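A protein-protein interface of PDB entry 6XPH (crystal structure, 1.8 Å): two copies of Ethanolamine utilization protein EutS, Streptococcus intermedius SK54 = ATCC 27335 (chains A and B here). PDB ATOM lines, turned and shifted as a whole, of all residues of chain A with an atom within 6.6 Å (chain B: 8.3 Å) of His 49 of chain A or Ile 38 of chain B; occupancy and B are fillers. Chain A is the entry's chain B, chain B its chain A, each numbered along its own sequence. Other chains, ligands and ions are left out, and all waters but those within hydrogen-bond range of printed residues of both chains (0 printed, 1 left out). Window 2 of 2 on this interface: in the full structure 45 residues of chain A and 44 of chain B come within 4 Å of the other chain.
Val 41 of chain B touches Ile 38 of chain A (CG1 to N, 3.9 Å). CD1 of Ile 38 of chain A touches CE1 of Tyr 42 of chain B (3.4 Å). Ile 38 of chain B touches Val 41 of chain A. Val 41 of chain A touches Val 41 of chain B. Ile 38 of chain B touches Tyr 42 of chain A (CD1 to CE1, 3.4 Å). Leu 45 of chain A touches Ile 38 of chain B (CD1 to CD1, 3.8 Å). CD1 of Ile 38 of chain B touches O of His 49 of chain A (3.6 Å). Gly 51 of chain A touches Ala 35 of chain B (O to O, 3.9 Å). Gly 51 of chain A touches Pro 37 of chain B. Ile 34 of chain B touches Ala 52 of chain A.
Of the printed residues of chain B, His 49 of chain A touches Ile 38 (3.6 Å). Of the printed residues of chain A, Ile 38 of chain B touches Val 41 (3.9 Å), Tyr 42 (3.4 Å), Leu 45 (3.8 Å) and His 49 (3.6 Å). Of the printed residues of chain B, Ile 38 of chain A touches Val 41 (3.9 Å) and Tyr 42 (3.4 Å). Of the printed residues of chain A, Ile 34 of chain B touches Ala 52 (3.5 Å). Of the printed residues of chain B, Leu 45 of chain A touches Ile 38 (3.8 Å). Printed residues of chain B within 4 Å of Ala 52 of chain A: Ile 34. The nearest printed residue of chain B that does not touch His 49 of chain A is Pro 37 of chain B (6.3 Å). The nearest printed residue of chain A that does not touch Ile 38 of chain B is Ile 38 of chain A (4.8 Å). The nearest printed residue of chain A that does not touch Ile 34 of chain B is Gly 51 of chain A (5.0 Å).
Of the 12 printed residues of chain B, 6 touch a printed residue of chain A. Hydrophobic or aromatic side chains of chain A within 4 Å of the printed part of chain B: Ile 38, Val 41, Tyr 42, Leu 45 and Ala 52. Among the printed residues, no Asp or Glu carboxylate lies within 4 Å of a Lys or Arg side-chain nitrogen of the other chain.
Ile 38 of chain A touches Val 41 of chain B, and with the chains exchanged Val 41 of chain A touches Ile 38 of chain B. Ile 38 of chain A touches Tyr 42 of chain B, and with the chains exchanged Tyr 42 of chain A touches Ile 38 of chain B. Val 41 of chain A touches its own counterpart, Val 41 of chain B. Leu 45 of chain A touches Ile 38 of chain B, but with the chains exchanged Ile 38 of chain A does not touch Leu 45 of chain B (4.05 Å). Positions printed for both chains: 38, 41, 42, 43 and 45.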
ATOM      1  N   ILE A  38       5.406   1.581  20.980  1.00  0.00           N
ATOM      2  CA  ILE A  38       6.108   0.388  21.523  1.00  0.00           C
ATOM      3  C   ILE A  38       6.785   0.769  22.842  1.00  0.00           C
ATOM      4  O   ILE A  38       6.554   0.082  23.832  1.00  0.00           O
ATOM      5  CB  ILE A  38       7.099  -0.212  20.513  1.00  0.00           C
ATOM      6  CG1 ILE A  38       6.444  -0.521  19.162  1.00  0.00           C
ATOM      7  CG2 ILE A  38       7.715  -1.450  21.148  1.00  0.00           C
ATOM      8  CD1 ILE A  38       7.413  -0.520  17.999  1.00  0.00           C
ATOM      9  N   VAL A  41       4.163   1.359  25.593  1.00  0.00           N
ATOM     10  CA  VAL A  41       3.630   0.103  26.168  1.00  0.00           C
ATOM     11  C   VAL A  41       4.688  -0.498  27.104  1.00  0.00           C
ATOM     12  O   VAL A  41       4.297  -0.917  28.176  1.00  0.00           O
ATOM     13  CB  VAL A  41       3.193  -0.905  25.091  1.00  0.00           C
ATOM     14  CG1 VAL A  41       2.939  -2.282  25.710  1.00  0.00           C
ATOM     15  CG2 VAL A  41       1.976  -0.407  24.357  1.00  0.00           C
ATOM     16  N   TYR A  42       5.980  -0.532  26.748  1.00  0.00           N
ATOM     17  CA  TYR A  42       6.969  -1.141  27.668  1.00  0.00           C
ATOM     18  C   TYR A  42       7.078  -0.333  28.959  1.00  0.00           C
ATOM     19  O   TYR A  42       7.200  -0.964  29.983  1.00  0.00           O
ATOM     20  CB  TYR A  42       8.335  -1.286  26.994  1.00  0.00           C
ATOM     21  CG  TYR A  42       8.429  -2.454  26.047  1.00  0.00           C
ATOM     22  CD1 TYR A  42       8.375  -3.745  26.511  1.00  0.00           C
ATOM     23  CD2 TYR A  42       8.707  -2.271  24.699  1.00  0.00           C
ATOM     24  CE1 TYR A  42       8.511  -4.840  25.662  1.00  0.00           C
ATOM     25  CE2 TYR A  42       8.856  -3.351  23.829  1.00  0.00           C
ATOM     26  CZ  TYR A  42       8.774  -4.639  24.322  1.00  0.00           C
ATOM     27  OH  TYR A  42       8.941  -5.695  23.469  1.00  0.00           O
ATOM     28  N   GLU A  43       6.931   0.985  28.921  1.00  0.00           N
ATOM     29  CA  GLU A  43       6.962   1.839  30.134  1.00  0.00           C
ATOM     30  C   GLU A  43       5.750   1.508  31.013  1.00  0.00           C
ATOM     31  O   GLU A  43       5.915   1.388  32.222  1.00  0.00           O
ATOM     32  CB  GLU A  43       6.976   3.334  29.820  1.00  0.00           C
ATOM     33  CG  GLU A  43       8.232   3.774  29.065  1.00  0.00           C
ATOM     34  CD  GLU A  43       8.482   5.265  28.839  1.00  0.00           C
ATOM     35  OE1 GLU A  43       7.571   6.076  29.122  1.00  0.00           O
ATOM     36  OE2 GLU A  43       9.607   5.615  28.399  1.00  0.00           O
ATOM     37  N   LEU A  45       4.124  -1.440  31.110  1.00  0.00           N
ATOM     38  CA  LEU A  45       4.345  -2.819  31.652  1.00  0.00           C
ATOM     39  C   LEU A  45       5.372  -2.791  32.787  1.00  0.00           C
ATOM     40  O   LEU A  45       5.257  -3.631  33.703  1.00  0.00           O
ATOM     41  CB  LEU A  45       4.820  -3.743  30.527  1.00  0.00           C
ATOM     42  CG  LEU A  45       3.743  -4.032  29.479  1.00  0.00           C
ATOM     43  CD1 LEU A  45       4.286  -4.919  28.393  1.00  0.00           C
ATOM     44  CD2 LEU A  45       2.533  -4.670  30.175  1.00  0.00           C
ATOM     45  N   GLY A  46       6.344  -1.884  32.720  1.00  0.00           N
ATOM     46  CA  GLY A  46       7.430  -1.785  33.714  1.00  0.00           C
ATOM     47  C   GLY A  46       8.337  -3.002  33.639  1.00  0.00           C
ATOM     48  O   GLY A  46       8.643  -3.417  32.497  1.00  0.00           O
ATOM     49  N   VAL A  47       8.731  -3.550  34.805  1.00  0.00           N
ATOM     50  CA  VAL A  47       9.659  -4.719  34.947  1.00  0.00           C
ATOM     51  C   VAL A  47       9.127  -5.943  34.189  1.00  0.00           C
ATOM     52  O   VAL A  47       9.953  -6.648  33.580  1.00  0.00           O
ATOM     53  CB  VAL A  47       9.948  -5.121  36.416  1.00  0.00           C
ATOM     54  CG1 VAL A  47      11.447  -5.229  36.634  1.00  0.00           C
ATOM     55  CG2 VAL A  47       9.316  -4.209  37.474  1.00  0.00           C
ATOM     56  N   ASP A  48       7.821  -6.216  34.240  1.00  0.00           N
ATOM     57  CA  ASP A  48       7.235  -7.481  33.717  1.00  0.00           C
ATOM     58  C   ASP A  48       6.768  -7.264  32.276  1.00  0.00           C
ATOM     59  O   ASP A  48       5.625  -6.817  32.086  1.00  0.00           O
ATOM     60  CB  ASP A  48       6.072  -8.022  34.572  1.00  0.00           C
ATOM     61  CG  ASP A  48       5.538  -9.382  34.089  1.00  0.00           C
ATOM     62  OD1 ASP A  48       6.128  -9.930  33.129  1.00  0.00           O
ATOM     63  OD2 ASP A  48       4.511  -9.865  34.634  1.00  0.00           O
ATOM     64  N   HIS A  49       7.606  -7.593  31.305  1.00  0.00           N
ATOM     65  CA  HIS A  49       7.277  -7.411  29.873  1.00  0.00           C
ATOM     66  C   HIS A  49       6.255  -8.451  29.422  1.00  0.00           C
ATOM     67  O   HIS A  49       5.759  -8.302  28.277  1.00  0.00           O
ATOM     68  CB  HIS A  49       8.549  -7.445  28.990  1.00  0.00           C
ATOM     69  CG  HIS A  49       9.414  -6.231  29.113  1.00  0.00           C
ATOM     70  ND1 HIS A  49      10.652  -6.130  28.475  1.00  0.00           N
ATOM     71  CD2 HIS A  49       9.230  -5.049  29.751  1.00  0.00           C
ATOM     72  CE1 HIS A  49      11.176  -4.941  28.713  1.00  0.00           C
ATOM     73  NE2 HIS A  49      10.334  -4.259  29.499  1.00  0.00           N
ATOM     74  N   GLU A  50       5.938  -9.455  30.262  1.00  0.00           N
ATOM     75  CA  GLU A  50       4.907 -10.471  29.925  1.00  0.00           C
ATOM     76  C   GLU A  50       3.562 -10.080  30.551  1.00  0.00           C
ATOM     77  O   GLU A  50       2.638 -10.860  30.437  1.00  0.00           O
ATOM     78  CB  GLU A  50       5.404 -11.850  30.368  1.00  0.00           C
ATOM     79  CG  GLU A  50       6.621 -12.280  29.563  1.00  0.00           C
ATOM     80  CD  GLU A  50       7.076 -13.704  29.825  1.00  0.00           C
ATOM     81  OE1 GLU A  50       7.055 -14.117  31.011  1.00  0.00           O
ATOM     82  OE2 GLU A  50       7.441 -14.396  28.839  1.00  0.00           O
ATOM     83  N   GLY A  51       3.465  -8.861  31.089  1.00  0.00           N
ATOM     84  CA  GLY A  51       2.276  -8.320  31.737  1.00  0.00           C
ATOM     85  C   GLY A  51       1.150  -8.014  30.775  1.00  0.00           C
ATOM     86  O   GLY A  51       1.337  -8.066  29.523  1.00  0.00           O
ATOM     87  N   ALA A  52      -0.018  -7.772  31.350  1.00  0.00           N
ATOM     88  CA  ALA A  52      -1.239  -7.395  30.613  1.00  0.00           C
ATOM     89  C   ALA A  52      -1.568  -5.955  30.943  1.00  0.00           C
ATOM     90  O   ALA A  52      -1.118  -5.473  31.997  1.00  0.00           O
ATOM     91  CB  ALA A  52      -2.383  -8.278  31.035  1.00  0.00           C
ATOM     92  N   ILE B  34      -6.118  -6.233  27.753  1.00  0.00           N
ATOM     93  CA  ILE B  34      -5.243  -6.405  26.572  1.00  0.00           C
ATOM     94  C   ILE B  34      -4.173  -7.399  26.988  1.00  0.00           C
ATOM     95  O   ILE B  34      -3.253  -7.051  27.772  1.00  0.00           O
ATOM     96  CB  ILE B  34      -4.673  -5.055  26.120  1.00  0.00           C
ATOM     97  CG1 ILE B  34      -5.753  -3.982  25.956  1.00  0.00           C
ATOM     98  CG2 ILE B  34      -3.844  -5.264  24.851  1.00  0.00           C
ATOM     99  CD1 ILE B  34      -5.225  -2.608  25.740  1.00  0.00           C
ATOM    100  N   ALA B  35      -4.336  -8.639  26.581  1.00  0.00           N
ATOM    101  CA  ALA B  35      -3.505  -9.747  27.083  1.00  0.00           C
ATOM    102  C   ALA B  35      -2.078  -9.644  26.531  1.00  0.00           C
ATOM    103  O   ALA B  35      -1.164  -9.999  27.236  1.00  0.00           O
ATOM    104  CB  ALA B  35      -4.134 -11.066  26.702  1.00  0.00           C
ATOM    105  N   ALA B  36      -1.899  -9.106  25.336  1.00  0.00           N
ATOM    106  CA  ALA B  36      -0.598  -9.078  24.628  1.00  0.00           C
ATOM    107  C   ALA B  36      -0.420  -7.700  24.019  1.00  0.00           C
ATOM    108  O   ALA B  36      -0.539  -7.535  22.801  1.00  0.00           O
ATOM    109  CB  ALA B  36      -0.540 -10.184  23.596  1.00  0.00           C
ATOM    110  N   PRO B  37      -0.189  -6.664  24.863  1.00  0.00           N
ATOM    111  CA  PRO B  37      -0.249  -5.279  24.398  1.00  0.00           C
ATOM    112  C   PRO B  37       0.860  -4.974  23.390  1.00  0.00           C
ATOM    113  O   PRO B  37       0.635  -4.192  22.527  1.00  0.00           O
ATOM    114  CB  PRO B  37      -0.166  -4.388  25.650  1.00  0.00           C
ATOM    115  CG  PRO B  37       0.335  -5.335  26.726  1.00  0.00           C
ATOM    116  CD  PRO B  37      -0.040  -6.750  26.331  1.00  0.00           C
ATOM    117  N   ILE B  38       2.028  -5.605  23.465  1.00  0.00           N
ATOM    118  CA  ILE B  38       3.077  -5.332  22.450  1.00  0.00           C
ATOM    119  C   ILE B  38       2.597  -5.842  21.081  1.00  0.00           C
ATOM    120  O   ILE B  38       2.692  -5.082  20.048  1.00  0.00           O
ATOM    121  CB  ILE B  38       4.417  -5.937  22.910  1.00  0.00           C
ATOM    122  CG1 ILE B  38       4.804  -5.462  24.318  1.00  0.00           C
ATOM    123  CG2 ILE B  38       5.475  -5.628  21.875  1.00  0.00           C
ATOM    124  CD1 ILE B  38       5.532  -6.487  25.156  1.00  0.00           C
ATOM    125  N   GLU B  39       2.039  -7.045  21.051  1.00  0.00           N
ATOM    126  CA  GLU B  39       1.477  -7.576  19.790  1.00  0.00           C
ATOM    127  C   GLU B  39       0.400  -6.629  19.258  1.00  0.00           C
ATOM    128  O   GLU B  39       0.323  -6.466  18.030  1.00  0.00           O
ATOM    129  CB  GLU B  39       0.856  -8.953  19.932  1.00  0.00           C
ATOM    130  CG  GLU B  39       1.847 -10.075  20.103  1.00  0.00           C
ATOM    131  CD  GLU B  39       1.104 -11.399  20.301  1.00  0.00           C
ATOM    132  OE1 GLU B  39      -0.061 -11.534  19.774  1.00  0.00           O
ATOM    133  OE2 GLU B  39       1.636 -12.259  21.057  1.00  0.00           O
ATOM    134  N   ALA B  40      -0.438  -6.127  20.146  1.00  0.00           N
ATOM    135  CA  ALA B  40      -1.550  -5.221  19.787  1.00  0.00           C
ATOM    136  C   ALA B  40      -0.998  -3.926  19.181  1.00  0.00           C
ATOM    137  O   ALA B  40      -1.518  -3.503  18.144  1.00  0.00           O
ATOM    138  CB  ALA B  40      -2.409  -4.949  20.973  1.00  0.00           C
ATOM    139  N   VAL B  41       0.069  -3.376  19.722  1.00  0.00           N
ATOM    140  CA  VAL B  41       0.657  -2.143  19.127  1.00  0.00           C
ATOM    141  C   VAL B  41       1.230  -2.441  17.740  1.00  0.00           C
ATOM    142  O   VAL B  41       0.967  -1.682  16.799  1.00  0.00           O
ATOM    143  CB  VAL B  41       1.691  -1.490  20.063  1.00  0.00           C
ATOM    144  CG1 VAL B  41       2.448  -0.394  19.327  1.00  0.00           C
ATOM    145  CG2 VAL B  41       1.000  -0.886  21.233  1.00  0.00           C
ATOM    146  N   TYR B  42       1.943  -3.554  17.547  1.00  0.00           N
ATOM    147  CA  TYR B  42       2.506  -3.852  16.205  1.00  0.00           C
ATOM    148  C   TYR B  42       1.375  -4.055  15.198  1.00  0.00           C
ATOM    149  O   TYR B  42       1.513  -3.634  14.017  1.00  0.00           O
ATOM    150  CB  TYR B  42       3.435  -5.065  16.285  1.00  0.00           C
ATOM    151  CG  TYR B  42       4.814  -4.725  16.765  1.00  0.00           C
ATOM    152  CD1 TYR B  42       5.612  -3.875  16.029  1.00  0.00           C
ATOM    153  CD2 TYR B  42       5.307  -5.213  17.961  1.00  0.00           C
ATOM    154  CE1 TYR B  42       6.895  -3.557  16.447  1.00  0.00           C
ATOM    155  CE2 TYR B  42       6.592  -4.923  18.383  1.00  0.00           C
ATOM    156  CZ  TYR B  42       7.390  -4.094  17.621  1.00  0.00           C
ATOM    157  OH  TYR B  42       8.646  -3.772  18.037  1.00  0.00           O
ATOM    158  N   GLU B  43       0.276  -4.710  15.631  1.00  0.00           N
ATOM    159  CA  GLU B  43      -0.913  -4.927  14.771  1.00  0.00           C
ATOM    160  C   GLU B  43      -1.476  -3.563  14.354  1.00  0.00           C
ATOM    161  O   GLU B  43      -1.855  -3.382  13.158  1.00  0.00           O
ATOM    162  CB  GLU B  43      -1.976  -5.822  15.432  1.00  0.00           C
ATOM    163  CG  GLU B  43      -1.665  -7.313  15.388  1.00  0.00           C
ATOM    164  CD  GLU B  43      -2.680  -8.245  16.053  1.00  0.00           C
ATOM    165  OE1 GLU B  43      -3.879  -7.878  16.122  1.00  0.00           O
ATOM    166  OE2 GLU B  43      -2.274  -9.346  16.503  1.00  0.00           O
ATOM    167  N   CYS B  44      -1.533  -2.602  15.246  1.00  0.00           N
ATOM    168  CA  CYS B  44      -2.098  -1.276  14.897  1.00  0.00           C
ATOM    169  C   CYS B  44      -1.103  -0.573  13.959  1.00  0.00           C
ATOM    170  O   CYS B  44      -1.508   0.075  12.999  1.00  0.00           O
ATOM    171  CB  CYS B  44      -2.427  -0.505  16.174  1.00  0.00           C
ATOM    172  SG  CYS B  44      -2.952   1.209  15.875  1.00  0.00           S
ATOM    173  N   LEU B  45       0.185  -0.658  14.224  1.00  0.00           N
ATOM    174  CA  LEU B  45       1.206   0.046  13.409  1.00  0.00           C
ATOM    175  C   LEU B  45       1.274  -0.585  12.008  1.00  0.00           C
ATOM    176  O   LEU B  45       1.617   0.133  11.066  1.00  0.00           O
ATOM    177  CB  LEU B  45       2.546  -0.041  14.111  1.00  0.00           C
ATOM    178  CG  LEU B  45       2.746   0.823  15.341  1.00  0.00           C
ATOM    179  CD1 LEU B  45       4.145   0.605  15.889  1.00  0.00           C
ATOM    180  CD2 LEU B  45       2.531   2.298  15.009  1.00  0.00           C
